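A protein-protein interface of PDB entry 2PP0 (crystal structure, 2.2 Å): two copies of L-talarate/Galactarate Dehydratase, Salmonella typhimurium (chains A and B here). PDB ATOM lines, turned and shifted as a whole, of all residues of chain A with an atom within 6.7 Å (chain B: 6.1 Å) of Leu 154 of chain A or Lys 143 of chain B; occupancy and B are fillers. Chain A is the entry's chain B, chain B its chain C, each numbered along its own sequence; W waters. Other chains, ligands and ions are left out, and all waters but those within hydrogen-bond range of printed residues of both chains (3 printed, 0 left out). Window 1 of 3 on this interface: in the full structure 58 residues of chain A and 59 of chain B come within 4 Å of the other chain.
Water W1 lies within hydrogen-bond range of the backbone carbonyl oxygen (O) of Ala 157 of chain A (2.8 Å), the backbone carbonyl oxygen (O) of Asp 107 of chain B (3.3 Å) and the backbone NH (N) of Ile 108 of chain B (3.4 Å).
Water W3 lies within hydrogen-bond range of the backbone carbonyl oxygen (O) of Ala 147 of chain A (2.9 Å) and the guanidinium group (NH1) of Arg 146 of chain B (3.1 Å).
Water W2 bridges the side-chain carboxylate (OD2) of Asp 107 of chain B and the backbone carbonyl oxygen (O) of Ala 157 of chain A.
NZ of Lys 143 of chain A lies within hydrogen-bond range of O of Leu 154 of chain B.
The side-chain carboxylate (OD2) of Asp 107 of chain B is in salt-bridge range of the side-chain amino group (NZ) of Lys 153 of chain A (2.8 Å).
NZ of Lys 143 of chain B sits at hydrogen-bond distance from O of Lys 153 of chain A, at 3.1 Å.
NZ of Lys 143 of chain B sits at hydrogen-bond distance from O of Leu 154 of chain A (2.9 Å).
The backbone NH (N) of Ala 157 of chain A lies within hydrogen-bond range of the side-chain carboxylate (OD1) of Asp 107 of chain B.
The backbone carbonyl oxygen of Lys 153 of chain A sits close to the backbone carbonyl oxygen of Asn 106 of chain B, 3.5 Å away.
Lys 143 of chain A touches Leu 154 of chain B, and with the chains exchanged Leu 154 of chain A touches Lys 143 of chain B.
Ala 147 of chain B touches its own counterpart, Ala 147 of chain A.
Of the 12 pairs that touch across the chains among the printed residues, 3 have their exchanged pair printed and touching as well.
Leu 154 of chain A touches just one residue of chain B: Lys 143 (2.9 Å).
Of the printed residues of chain A, Arg 146 of chain B touches Ala 147 (3.3 Å) and Leu 149 (3.9 Å).
Of the printed residues of chain B, Ala 157 of chain A touches Asp 107.
Trp 140 of chain A touches none of the printed residues of chain B.
The nearest residue of chain B that does not touch Leu 154 of chain A is Leu 154 of chain B (4.1 Å).
The nearest residue of chain A that does not touch Lys 143 of chain B is Gly 156 of chain A (4.02 Å).
The nearest printed residue of chain B that does not touch Lys 153 of chain A is Ile 108 of chain B (6.4 Å).
Printed residues of chain A that touch a printed residue of chain B: Lys 143, Ala 147, Leu 149, Lys 153, Leu 154, Gly 156 and Ala 157.
Of the 16 printed residues of chain B, 6 touch a printed residue of chain A.
Printed residues of chain B that touch a printed residue of chain A: Asn 106, Asp 107, Lys 143, Arg 146, Ala 147 and Leu 154.
Along chain B the printed residues that touch a printed residue of chain A span positions 106 to 154.
Among the printed residues, 12 pairs touch across the chains.
Among the printed residues, Asp or Glu carboxylates within 4 Å of a Lys or Arg side-chain nitrogen of the other chain: Lys 153 of chain A with Asp 107 of chain B.
Among the printed residues, pairs that only touch across the chains: Gly 156 of chain A with Asn 106 of chain B (3.3 Å), Ala 147 of chain A with Arg 146 of chain B (3.3 Å), Leu 149 of chain A with Asn 106 of chain B (3.4 Å), Ala 147 of chain A with Ala 147 of chain B (3.8 Å), Gly 156 of chain A with Asp 107 of chain B (3.8 Å) and Leu 149 of chain A with Arg 146 of chain B (3.9 Å).
The backbone carbonyl oxygen (O) of Ala 144 of chain A is in hydrogen-bond range of the backbone NH (N) of Leu 149 of chain A (3.0 Å).
The backbone carbonyl oxygen (O) of Ala 152 of chain A is in hydrogen-bond range of the backbone NH (N) of Ala 157 of chain A (3.3 Å).
NZ of Lys 143 of chain B sits at hydrogen-bond distance from O of Asn 106 of chain B (2.8 Å).
The guanidinium group (NE) of Arg 146 of chain B sits close to the side-chain amide nitrogen (ND2) of Asn 106 of chain B (3.3 Å).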
ATOM      1  N   LEU A 139      14.424  18.277  -6.370  1.00  0.00           N
ATOM      2  CA  LEU A 139      14.485  19.731  -6.369  1.00  0.00           C
ATOM      3  C   LEU A 139      15.006  20.251  -5.029  1.00  0.00           C
ATOM      4  O   LEU A 139      15.751  21.230  -4.995  1.00  0.00           O
ATOM      5  CB  LEU A 139      13.111  20.327  -6.683  1.00  0.00           C
ATOM      6  CG  LEU A 139      12.628  20.130  -8.122  1.00  0.00           C
ATOM      7  CD1 LEU A 139      11.248  20.759  -8.279  1.00  0.00           C
ATOM      8  CD2 LEU A 139      13.620  20.773  -9.098  1.00  0.00           C
ATOM      9  N   TRP A 140      14.626  19.605  -3.929  1.00  0.00           N
ATOM     10  CA  TRP A 140      15.125  20.018  -2.616  1.00  0.00           C
ATOM     11  C   TRP A 140      16.617  19.678  -2.491  1.00  0.00           C
ATOM     12  O   TRP A 140      17.391  20.433  -1.882  1.00  0.00           O
ATOM     13  CB  TRP A 140      14.347  19.336  -1.491  1.00  0.00           C
ATOM     14  CG  TRP A 140      13.082  20.051  -1.127  1.00  0.00           C
ATOM     15  CD1 TRP A 140      11.804  19.724  -1.502  1.00  0.00           C
ATOM     16  CD2 TRP A 140      12.976  21.232  -0.326  1.00  0.00           C
ATOM     17  NE1 TRP A 140      10.909  20.634  -0.978  1.00  0.00           N
ATOM     18  CE2 TRP A 140      11.603  21.570  -0.252  1.00  0.00           C
ATOM     19  CE3 TRP A 140      13.910  22.042   0.339  1.00  0.00           C
ATOM     20  CZ2 TRP A 140      11.144  22.682   0.460  1.00  0.00           C
ATOM     21  CZ3 TRP A 140      13.452  23.152   1.049  1.00  0.00           C
ATOM     22  CH2 TRP A 140      12.081  23.460   1.103  1.00  0.00           C
ATOM     23  N   ASP A 141      17.007  18.540  -3.063  1.00  0.00           N
ATOM     24  CA  ASP A 141      18.401  18.088  -3.061  1.00  0.00           C
ATOM     25  C   ASP A 141      19.233  19.141  -3.794  1.00  0.00           C
ATOM     26  O   ASP A 141      20.300  19.542  -3.327  1.00  0.00           O
ATOM     27  CB  ASP A 141      18.507  16.729  -3.777  1.00  0.00           C
ATOM     28  CG  ASP A 141      19.940  16.215  -3.886  1.00  0.00           C
ATOM     29  OD1 ASP A 141      20.590  15.966  -2.841  1.00  0.00           O
ATOM     30  OD2 ASP A 141      20.412  16.049  -5.031  1.00  0.00           O
ATOM     31  N   MET A 142      18.717  19.599  -4.933  1.00  0.00           N
ATOM     32  CA  MET A 142      19.392  20.606  -5.745  1.00  0.00           C
ATOM     33  C   MET A 142      19.519  21.937  -5.009  1.00  0.00           C
ATOM     34  O   MET A 142      20.599  22.538  -4.984  1.00  0.00           O
ATOM     35  CB  MET A 142      18.640  20.827  -7.070  1.00  0.00           C
ATOM     36  CG  MET A 142      19.258  21.907  -7.970  1.00  0.00           C
ATOM     37  SD  MET A 142      18.342  22.310  -9.487  1.00  0.00           S
ATOM     38  CE  MET A 142      18.814  20.899 -10.457  1.00  0.00           C
ATOM     39  N   LYS A 143      18.428  22.403  -4.407  1.00  0.00           N
ATOM     40  CA  LYS A 143      18.471  23.678  -3.697  1.00  0.00           C
ATOM     41  C   LYS A 143      19.479  23.676  -2.554  1.00  0.00           C
ATOM     42  O   LYS A 143      20.173  24.672  -2.334  1.00  0.00           O
ATOM     43  CB  LYS A 143      17.083  24.067  -3.167  1.00  0.00           C
ATOM     44  CG  LYS A 143      17.104  25.393  -2.423  1.00  0.00           C
ATOM     45  CD  LYS A 143      15.717  25.919  -2.101  1.00  0.00           C
ATOM     46  CE  LYS A 143      15.009  26.433  -3.339  1.00  0.00           C
ATOM     47  NZ  LYS A 143      13.747  27.134  -2.965  1.00  0.00           N
ATOM     48  N   ALA A 144      19.565  22.565  -1.828  1.00  0.00           N
ATOM     49  CA  ALA A 144      20.505  22.448  -0.720  1.00  0.00           C
ATOM     50  C   ALA A 144      21.930  22.517  -1.263  1.00  0.00           C
ATOM     51  O   ALA A 144      22.775  23.244  -0.732  1.00  0.00           O
ATOM     52  CB  ALA A 144      20.295  21.130   0.027  1.00  0.00           C
ATOM     53  N   LYS A 145      22.190  21.754  -2.324  1.00  0.00           N
ATOM     54  CA  LYS A 145      23.506  21.741  -2.950  1.00  0.00           C
ATOM     55  C   LYS A 145      23.864  23.133  -3.458  1.00  0.00           C
ATOM     56  O   LYS A 145      25.019  23.544  -3.394  1.00  0.00           O
ATOM     57  CB  LYS A 145      23.536  20.735  -4.106  1.00  0.00           C
ATOM     58  CG  LYS A 145      23.496  19.291  -3.648  1.00  0.00           C
ATOM     59  CD  LYS A 145      23.368  18.320  -4.817  1.00  0.00           C
ATOM     60  CE  LYS A 145      23.463  16.874  -4.337  1.00  0.00           C
ATOM     61  NZ  LYS A 145      23.134  15.899  -5.427  1.00  0.00           N
ATOM     62  N   ALA A 147      23.111  25.806  -2.096  1.00  0.00           N
ATOM     63  CA  ALA A 147      23.499  26.583  -0.919  1.00  0.00           C
ATOM     64  C   ALA A 147      24.781  26.004  -0.306  1.00  0.00           C
ATOM     65  O   ALA A 147      25.337  26.564   0.648  1.00  0.00           O
ATOM     66  CB  ALA A 147      22.374  26.561   0.116  1.00  0.00           C
ATOM     67  N   LEU A 149      25.031  23.097   1.261  1.00  0.00           N
ATOM     68  CA  LEU A 149      24.678  22.577   2.577  1.00  0.00           C
ATOM     69  C   LEU A 149      23.973  21.239   2.538  1.00  0.00           C
ATOM     70  O   LEU A 149      23.343  20.889   1.547  1.00  0.00           O
ATOM     71  CB  LEU A 149      23.702  23.520   3.282  1.00  0.00           C
ATOM     72  CG  LEU A 149      23.983  24.993   3.524  1.00  0.00           C
ATOM     73  CD1 LEU A 149      22.678  25.694   3.906  1.00  0.00           C
ATOM     74  CD2 LEU A 149      25.025  25.125   4.614  1.00  0.00           C
ATOM     75  N   PRO A 150      24.098  20.463   3.622  1.00  0.00           N
ATOM     76  CA  PRO A 150      23.413  19.173   3.676  1.00  0.00           C
ATOM     77  C   PRO A 150      21.946  19.639   3.725  1.00  0.00           C
ATOM     78  O   PRO A 150      21.674  20.755   4.166  1.00  0.00           O
ATOM     79  CB  PRO A 150      23.872  18.600   5.012  1.00  0.00           C
ATOM     80  CG  PRO A 150      25.266  19.153   5.145  1.00  0.00           C
ATOM     81  CD  PRO A 150      25.095  20.582   4.702  1.00  0.00           C
ATOM     82  N   LEU A 151      21.003  18.815   3.287  1.00  0.00           N
ATOM     83  CA  LEU A 151      19.603  19.240   3.293  1.00  0.00           C
ATOM     84  C   LEU A 151      19.109  19.716   4.657  1.00  0.00           C
ATOM     85  O   LEU A 151      18.410  20.725   4.753  1.00  0.00           O
ATOM     86  CB  LEU A 151      18.699  18.104   2.794  1.00  0.00           C
ATOM     87  CG  LEU A 151      17.193  18.383   2.889  1.00  0.00           C
ATOM     88  CD1 LEU A 151      16.823  19.576   2.034  1.00  0.00           C
ATOM     89  CD2 LEU A 151      16.425  17.147   2.414  1.00  0.00           C
ATOM     90  N   ALA A 152      19.460  18.983   5.707  1.00  0.00           N
ATOM     91  CA  ALA A 152      19.041  19.329   7.060  1.00  0.00           C
ATOM     92  C   ALA A 152      19.417  20.766   7.425  1.00  0.00           C
ATOM     93  O   ALA A 152      18.679  21.447   8.137  1.00  0.00           O
ATOM     94  CB  ALA A 152      19.663  18.352   8.059  1.00  0.00           C
ATOM     95  N   LYS A 153      20.563  21.223   6.929  1.00  0.00           N
ATOM     96  CA  LYS A 153      21.034  22.575   7.214  1.00  0.00           C
ATOM     97  C   LYS A 153      20.282  23.608   6.397  1.00  0.00           C
ATOM     98  O   LYS A 153      20.044  24.718   6.868  1.00  0.00           O
ATOM     99  CB  LYS A 153      22.540  22.668   6.955  1.00  0.00           C
ATOM    100  CG  LYS A 153      23.344  21.870   7.970  1.00  0.00           C
ATOM    101  CD  LYS A 153      23.192  22.465   9.367  1.00  0.00           C
ATOM    102  CE  LYS A 153      23.959  21.654  10.395  1.00  0.00           C
ATOM    103  NZ  LYS A 153      23.944  22.317  11.732  1.00  0.00           N
ATOM    104  N   LEU A 154      19.908  23.251   5.171  1.00  0.00           N
ATOM    105  CA  LEU A 154      19.132  24.167   4.334  1.00  0.00           C
ATOM    106  C   LEU A 154      17.785  24.393   5.035  1.00  0.00           C
ATOM    107  O   LEU A 154      17.267  25.517   5.090  1.00  0.00           O
ATOM    108  CB  LEU A 154      18.873  23.552   2.956  1.00  0.00           C
ATOM    109  CG  LEU A 154      17.870  24.326   2.093  1.00  0.00           C
ATOM    110  CD1 LEU A 154      18.523  25.589   1.593  1.00  0.00           C
ATOM    111  CD2 LEU A 154      17.402  23.476   0.917  1.00  0.00           C
ATOM    112  N   LEU A 155      17.220  23.305   5.557  1.00  0.00           N
ATOM    113  CA  LEU A 155      15.939  23.349   6.265  1.00  0.00           C
ATOM    114  C   LEU A 155      16.114  24.009   7.626  1.00  0.00           C
ATOM    115  O   LEU A 155      15.205  24.681   8.129  1.00  0.00           O
ATOM    116  CB  LEU A 155      15.412  21.932   6.489  1.00  0.00           C
ATOM    117  CG  LEU A 155      15.087  21.083   5.263  1.00  0.00           C
ATOM    118  CD1 LEU A 155      14.706  19.687   5.718  1.00  0.00           C
ATOM    119  CD2 LEU A 155      13.961  21.730   4.478  1.00  0.00           C
ATOM    120  N   GLY A 156      17.290  23.807   8.215  1.00  0.00           N
ATOM    121  CA  GLY A 156      17.573  24.357   9.530  1.00  0.00           C
ATOM    122  C   GLY A 156      17.426  23.193  10.486  1.00  0.00           C
ATOM    123  O   GLY A 156      16.341  22.627  10.615  1.00  0.00           O
ATOM    124  N   ALA A 157      18.514  22.819  11.144  1.00  0.00           N
ATOM    125  CA  ALA A 157      18.495  21.690  12.054  1.00  0.00           C
ATOM    126  C   ALA A 157      18.397  22.053  13.529  1.00  0.00           C
ATOM    127  O   ALA A 157      18.781  23.145  13.950  1.00  0.00           O
ATOM    128  CB  ALA A 157      19.733  20.830  11.821  1.00  0.00           C
ATOM    129  N   PRO B 105      24.840  29.478  11.654  1.00  0.00           N
ATOM    130  CA  PRO B 105      23.775  30.381  11.201  1.00  0.00           C
ATOM    131  C   PRO B 105      22.636  29.754  10.395  1.00  0.00           C
ATOM    132  O   PRO B 105      21.611  30.394  10.171  1.00  0.00           O
ATOM    133  CB  PRO B 105      24.535  31.417  10.390  1.00  0.00           C
ATOM    134  CG  PRO B 105      25.638  30.588   9.770  1.00  0.00           C
ATOM    135  CD  PRO B 105      26.104  29.755  10.942  1.00  0.00           C
ATOM    136  N   ASN B 106      22.813  28.512   9.953  1.00  0.00           N
ATOM    137  CA  ASN B 106      21.778  27.858   9.156  1.00  0.00           C
ATOM    138  C   ASN B 106      20.661  27.258   9.997  1.00  0.00           C
ATOM    139  O   ASN B 106      19.574  26.974   9.483  1.00  0.00           O
ATOM    140  CB  ASN B 106      22.398  26.767   8.277  1.00  0.00           C
ATOM    141  CG  ASN B 106      23.434  27.314   7.319  1.00  0.00           C
ATOM    142  OD1 ASN B 106      24.628  27.057   7.466  1.00  0.00           O
ATOM    143  ND2 ASN B 106      22.984  28.078   6.334  1.00  0.00           N
ATOM    144  N   ASP B 107      20.927  27.055  11.282  1.00  0.00           N
ATOM    145  CA  ASP B 107      19.929  26.483  12.176  1.00  0.00           C
ATOM    146  C   ASP B 107      19.118  27.615  12.790  1.00  0.00           C
ATOM    147  O   ASP B 107      19.145  27.840  13.999  1.00  0.00           O
ATOM    148  CB  ASP B 107      20.628  25.640  13.252  1.00  0.00           C
ATOM    149  CG  ASP B 107      21.320  24.416  12.664  1.00  0.00           C
ATOM    150  OD1 ASP B 107      20.963  24.021  11.535  1.00  0.00           O
ATOM    151  OD2 ASP B 107      22.210  23.839  13.324  1.00  0.00           O
ATOM    152  N   ILE B 108      18.387  28.318  11.930  1.00  0.00           N
ATOM    153  CA  ILE B 108      17.596  29.468  12.330  1.00  0.00           C
ATOM    154  C   ILE B 108      16.608  29.238  13.469  1.00  0.00           C
ATOM    155  O   ILE B 108      16.623  29.974  14.456  1.00  0.00           O
ATOM    156  CB  ILE B 108      16.880  30.064  11.096  1.00  0.00           C
ATOM    157  CG1 ILE B 108      17.940  30.497  10.068  1.00  0.00           C
ATOM    158  CG2 ILE B 108      16.008  31.249  11.511  1.00  0.00           C
ATOM    159  CD1 ILE B 108      17.385  31.143   8.803  1.00  0.00           C
ATOM    160  N   ALA B 138      17.970  38.730   9.427  1.00  0.00           N
ATOM    161  CA  ALA B 138      19.350  38.757   8.946  1.00  0.00           C
ATOM    162  C   ALA B 138      19.817  37.328   8.624  1.00  0.00           C
ATOM    163  O   ALA B 138      20.526  37.113   7.651  1.00  0.00           O
ATOM    164  CB  ALA B 138      20.260  39.388   9.993  1.00  0.00           C
ATOM    165  N   LEU B 139      19.407  36.351   9.430  1.00  0.00           N
ATOM    166  CA  LEU B 139      19.805  34.963   9.191  1.00  0.00           C
ATOM    167  C   LEU B 139      19.202  34.417   7.897  1.00  0.00           C
ATOM    168  O   LEU B 139      19.842  33.635   7.188  1.00  0.00           O
ATOM    169  CB  LEU B 139      19.411  34.080  10.379  1.00  0.00           C
ATOM    170  CG  LEU B 139      20.139  34.430  11.684  1.00  0.00           C
ATOM    171  CD1 LEU B 139      19.539  33.661  12.857  1.00  0.00           C
ATOM    172  CD2 LEU B 139      21.630  34.117  11.533  1.00  0.00           C
ATOM    173  N   TRP B 140      17.978  34.830   7.583  1.00  0.00           N
ATOM    174  CA  TRP B 140      17.325  34.391   6.355  1.00  0.00           C
ATOM    175  C   TRP B 140      17.993  35.082   5.173  1.00  0.00           C
ATOM    176  O   TRP B 140      18.163  34.490   4.111  1.00  0.00           O
ATOM    177  CB  TRP B 140      15.831  34.731   6.374  1.00  0.00           C
ATOM    178  CG  TRP B 140      14.997  33.700   7.064  1.00  0.00           C
ATOM    179  CD1 TRP B 140      14.484  33.764   8.331  1.00  0.00           C
ATOM    180  CD2 TRP B 140      14.593  32.435   6.532  1.00  0.00           C
ATOM    181  NE1 TRP B 140      13.785  32.614   8.619  1.00  0.00           N
ATOM    182  CE2 TRP B 140      13.837  31.782   7.532  1.00  0.00           C
ATOM    183  CE3 TRP B 140      14.800  31.786   5.306  1.00  0.00           C
ATOM    184  CZ2 TRP B 140      13.284  30.510   7.342  1.00  0.00           C
ATOM    185  CZ3 TRP B 140      14.250  30.520   5.118  1.00  0.00           C
ATOM    186  CH2 TRP B 140      13.501  29.897   6.132  1.00  0.00           C
ATOM    187  N   ASP B 141      18.350  36.348   5.367  1.00  0.00           N
ATOM    188  CA  ASP B 141      19.033  37.130   4.338  1.00  0.00           C
ATOM    189  C   ASP B 141      20.350  36.419   4.036  1.00  0.00           C
ATOM    190  O   ASP B 141      20.731  36.262   2.875  1.00  0.00           O
ATOM    191  CB  ASP B 141      19.298  38.550   4.863  1.00  0.00           C
ATOM    192  CG  ASP B 141      20.048  39.423   3.874  1.00  0.00           C
ATOM    193  OD1 ASP B 141      19.505  39.724   2.788  1.00  0.00           O
ATOM    194  OD2 ASP B 141      21.189  39.822   4.193  1.00  0.00           O
ATOM    195  N   MET B 142      21.037  35.971   5.085  1.00  0.00           N
ATOM    196  CA  MET B 142      22.317  35.277   4.911  1.00  0.00           C
ATOM    197  C   MET B 142      22.147  33.956   4.164  1.00  0.00           C
ATOM    198  O   MET B 142      22.872  33.683   3.215  1.00  0.00           O
ATOM    199  CB  MET B 142      22.991  35.005   6.272  1.00  0.00           C
ATOM    200  CG  MET B 142      24.419  34.434   6.180  1.00  0.00           C
ATOM    201  SD  MET B 142      25.144  33.797   7.742  1.00  0.00           S
ATOM    202  CE  MET B 142      25.427  35.301   8.566  1.00  0.00           C
ATOM    203  N   LYS B 143      21.194  33.129   4.584  1.00  0.00           N
ATOM    204  CA  LYS B 143      21.005  31.844   3.907  1.00  0.00           C
ATOM    205  C   LYS B 143      20.720  32.019   2.415  1.00  0.00           C
ATOM    206  O   LYS B 143      21.242  31.267   1.593  1.00  0.00           O
ATOM    207  CB  LYS B 143      19.872  31.033   4.553  1.00  0.00           C
ATOM    208  CG  LYS B 143      19.751  29.611   3.982  1.00  0.00           C
ATOM    209  CD  LYS B 143      18.793  28.721   4.791  1.00  0.00           C
ATOM    210  CE  LYS B 143      19.361  28.402   6.163  1.00  0.00           C
ATOM    211  NZ  LYS B 143      18.552  27.392   6.905  1.00  0.00           N
ATOM    212  N   ALA B 144      19.895  33.003   2.066  1.00  0.00           N
ATOM    213  CA  ALA B 144      19.566  33.249   0.661  1.00  0.00           C
ATOM    214  C   ALA B 144      20.824  33.633  -0.115  1.00  0.00           C
ATOM    215  O   ALA B 144      21.035  33.177  -1.239  1.00  0.00           O
ATOM    216  CB  ALA B 144      18.517  34.365   0.540  1.00  0.00           C
ATOM    217  N   LYS B 145      21.657  34.475   0.491  1.00  0.00           N
ATOM    218  CA  LYS B 145      22.896  34.911  -0.150  1.00  0.00           C
ATOM    219  C   LYS B 145      23.828  33.719  -0.300  1.00  0.00           C
ATOM    220  O   LYS B 145      24.508  33.572  -1.307  1.00  0.00           O
ATOM    221  CB  LYS B 145      23.557  36.018   0.688  1.00  0.00           C
ATOM    222  CG  LYS B 145      22.832  37.351   0.587  1.00  0.00           C
ATOM    223  CD  LYS B 145      23.334  38.338   1.638  1.00  0.00           C
ATOM    224  CE  LYS B 145      22.745  39.727   1.441  1.00  0.00           C
ATOM    225  NZ  LYS B 145      23.038  40.590   2.635  1.00  0.00           N
ATOM    226  N   ARG B 146      23.843  32.863   0.712  1.00  0.00           N
ATOM    227  CA  ARG B 146      24.667  31.670   0.684  1.00  0.00           C
ATOM    228  C   ARG B 146      24.280  30.813  -0.529  1.00  0.00           C
ATOM    229  O   ARG B 146      25.130  30.160  -1.136  1.00  0.00           O
ATOM    230  CB  ARG B 146      24.461  30.869   1.975  1.00  0.00           C
ATOM    231  CG  ARG B 146      25.276  29.586   2.056  1.00  0.00           C
ATOM    232  CD  ARG B 146      24.985  28.845   3.343  1.00  0.00           C
ATOM    233  NE  ARG B 146      25.293  29.637   4.533  1.00  0.00           N
ATOM    234  CZ  ARG B 146      26.508  29.767   5.058  1.00  0.00           C
ATOM    235  NH1 ARG B 146      27.548  29.154   4.504  1.00  0.00           N
ATOM    236  NH2 ARG B 146      26.681  30.503   6.145  1.00  0.00           N
ATOM    237  N   ALA B 147      22.998  30.835  -0.885  1.00  0.00           N
ATOM    238  CA  ALA B 147      22.496  30.056  -2.022  1.00  0.00           C
ATOM    239  C   ALA B 147      22.524  30.850  -3.328  1.00  0.00           C
ATOM    240  O   ALA B 147      22.165  30.324  -4.384  1.00  0.00           O
ATOM    241  CB  ALA B 147      21.063  29.581  -1.735  1.00  0.00           C
ATOM    242  N   GLY B 148      22.947  32.111  -3.252  1.00  0.00           N
ATOM    243  CA  GLY B 148      22.998  32.957  -4.435  1.00  0.00           C
ATOM    244  C   GLY B 148      21.611  33.234  -4.989  1.00  0.00           C
ATOM    245  O   GLY B 148      21.409  33.250  -6.209  1.00  0.00           O
ATOM    246  N   LEU B 154      14.693  31.562  -2.474  1.00  0.00           N
ATOM    247  CA  LEU B 154      15.157  30.600  -1.472  1.00  0.00           C
ATOM    248  C   LEU B 154      13.921  29.926  -0.866  1.00  0.00           C
ATOM    249  O   LEU B 154      13.904  28.715  -0.638  1.00  0.00           O
ATOM    250  CB  LEU B 154      15.937  31.298  -0.354  1.00  0.00           C
ATOM    251  CG  LEU B 154      16.269  30.401   0.846  1.00  0.00           C
ATOM    252  CD1 LEU B 154      17.285  29.354   0.431  1.00  0.00           C
ATOM    253  CD2 LEU B 154      16.810  31.244   2.005  1.00  0.00           C
HETATM  254  O   HOH W   1      17.251  25.322  13.092  1.00  0.00           O
HETATM  255  O   HOH W   2      21.582  21.342  15.005  1.00  0.00           O
HETATM  256  O   HOH W   3      27.622  27.027   2.316  1.00  0.00           O
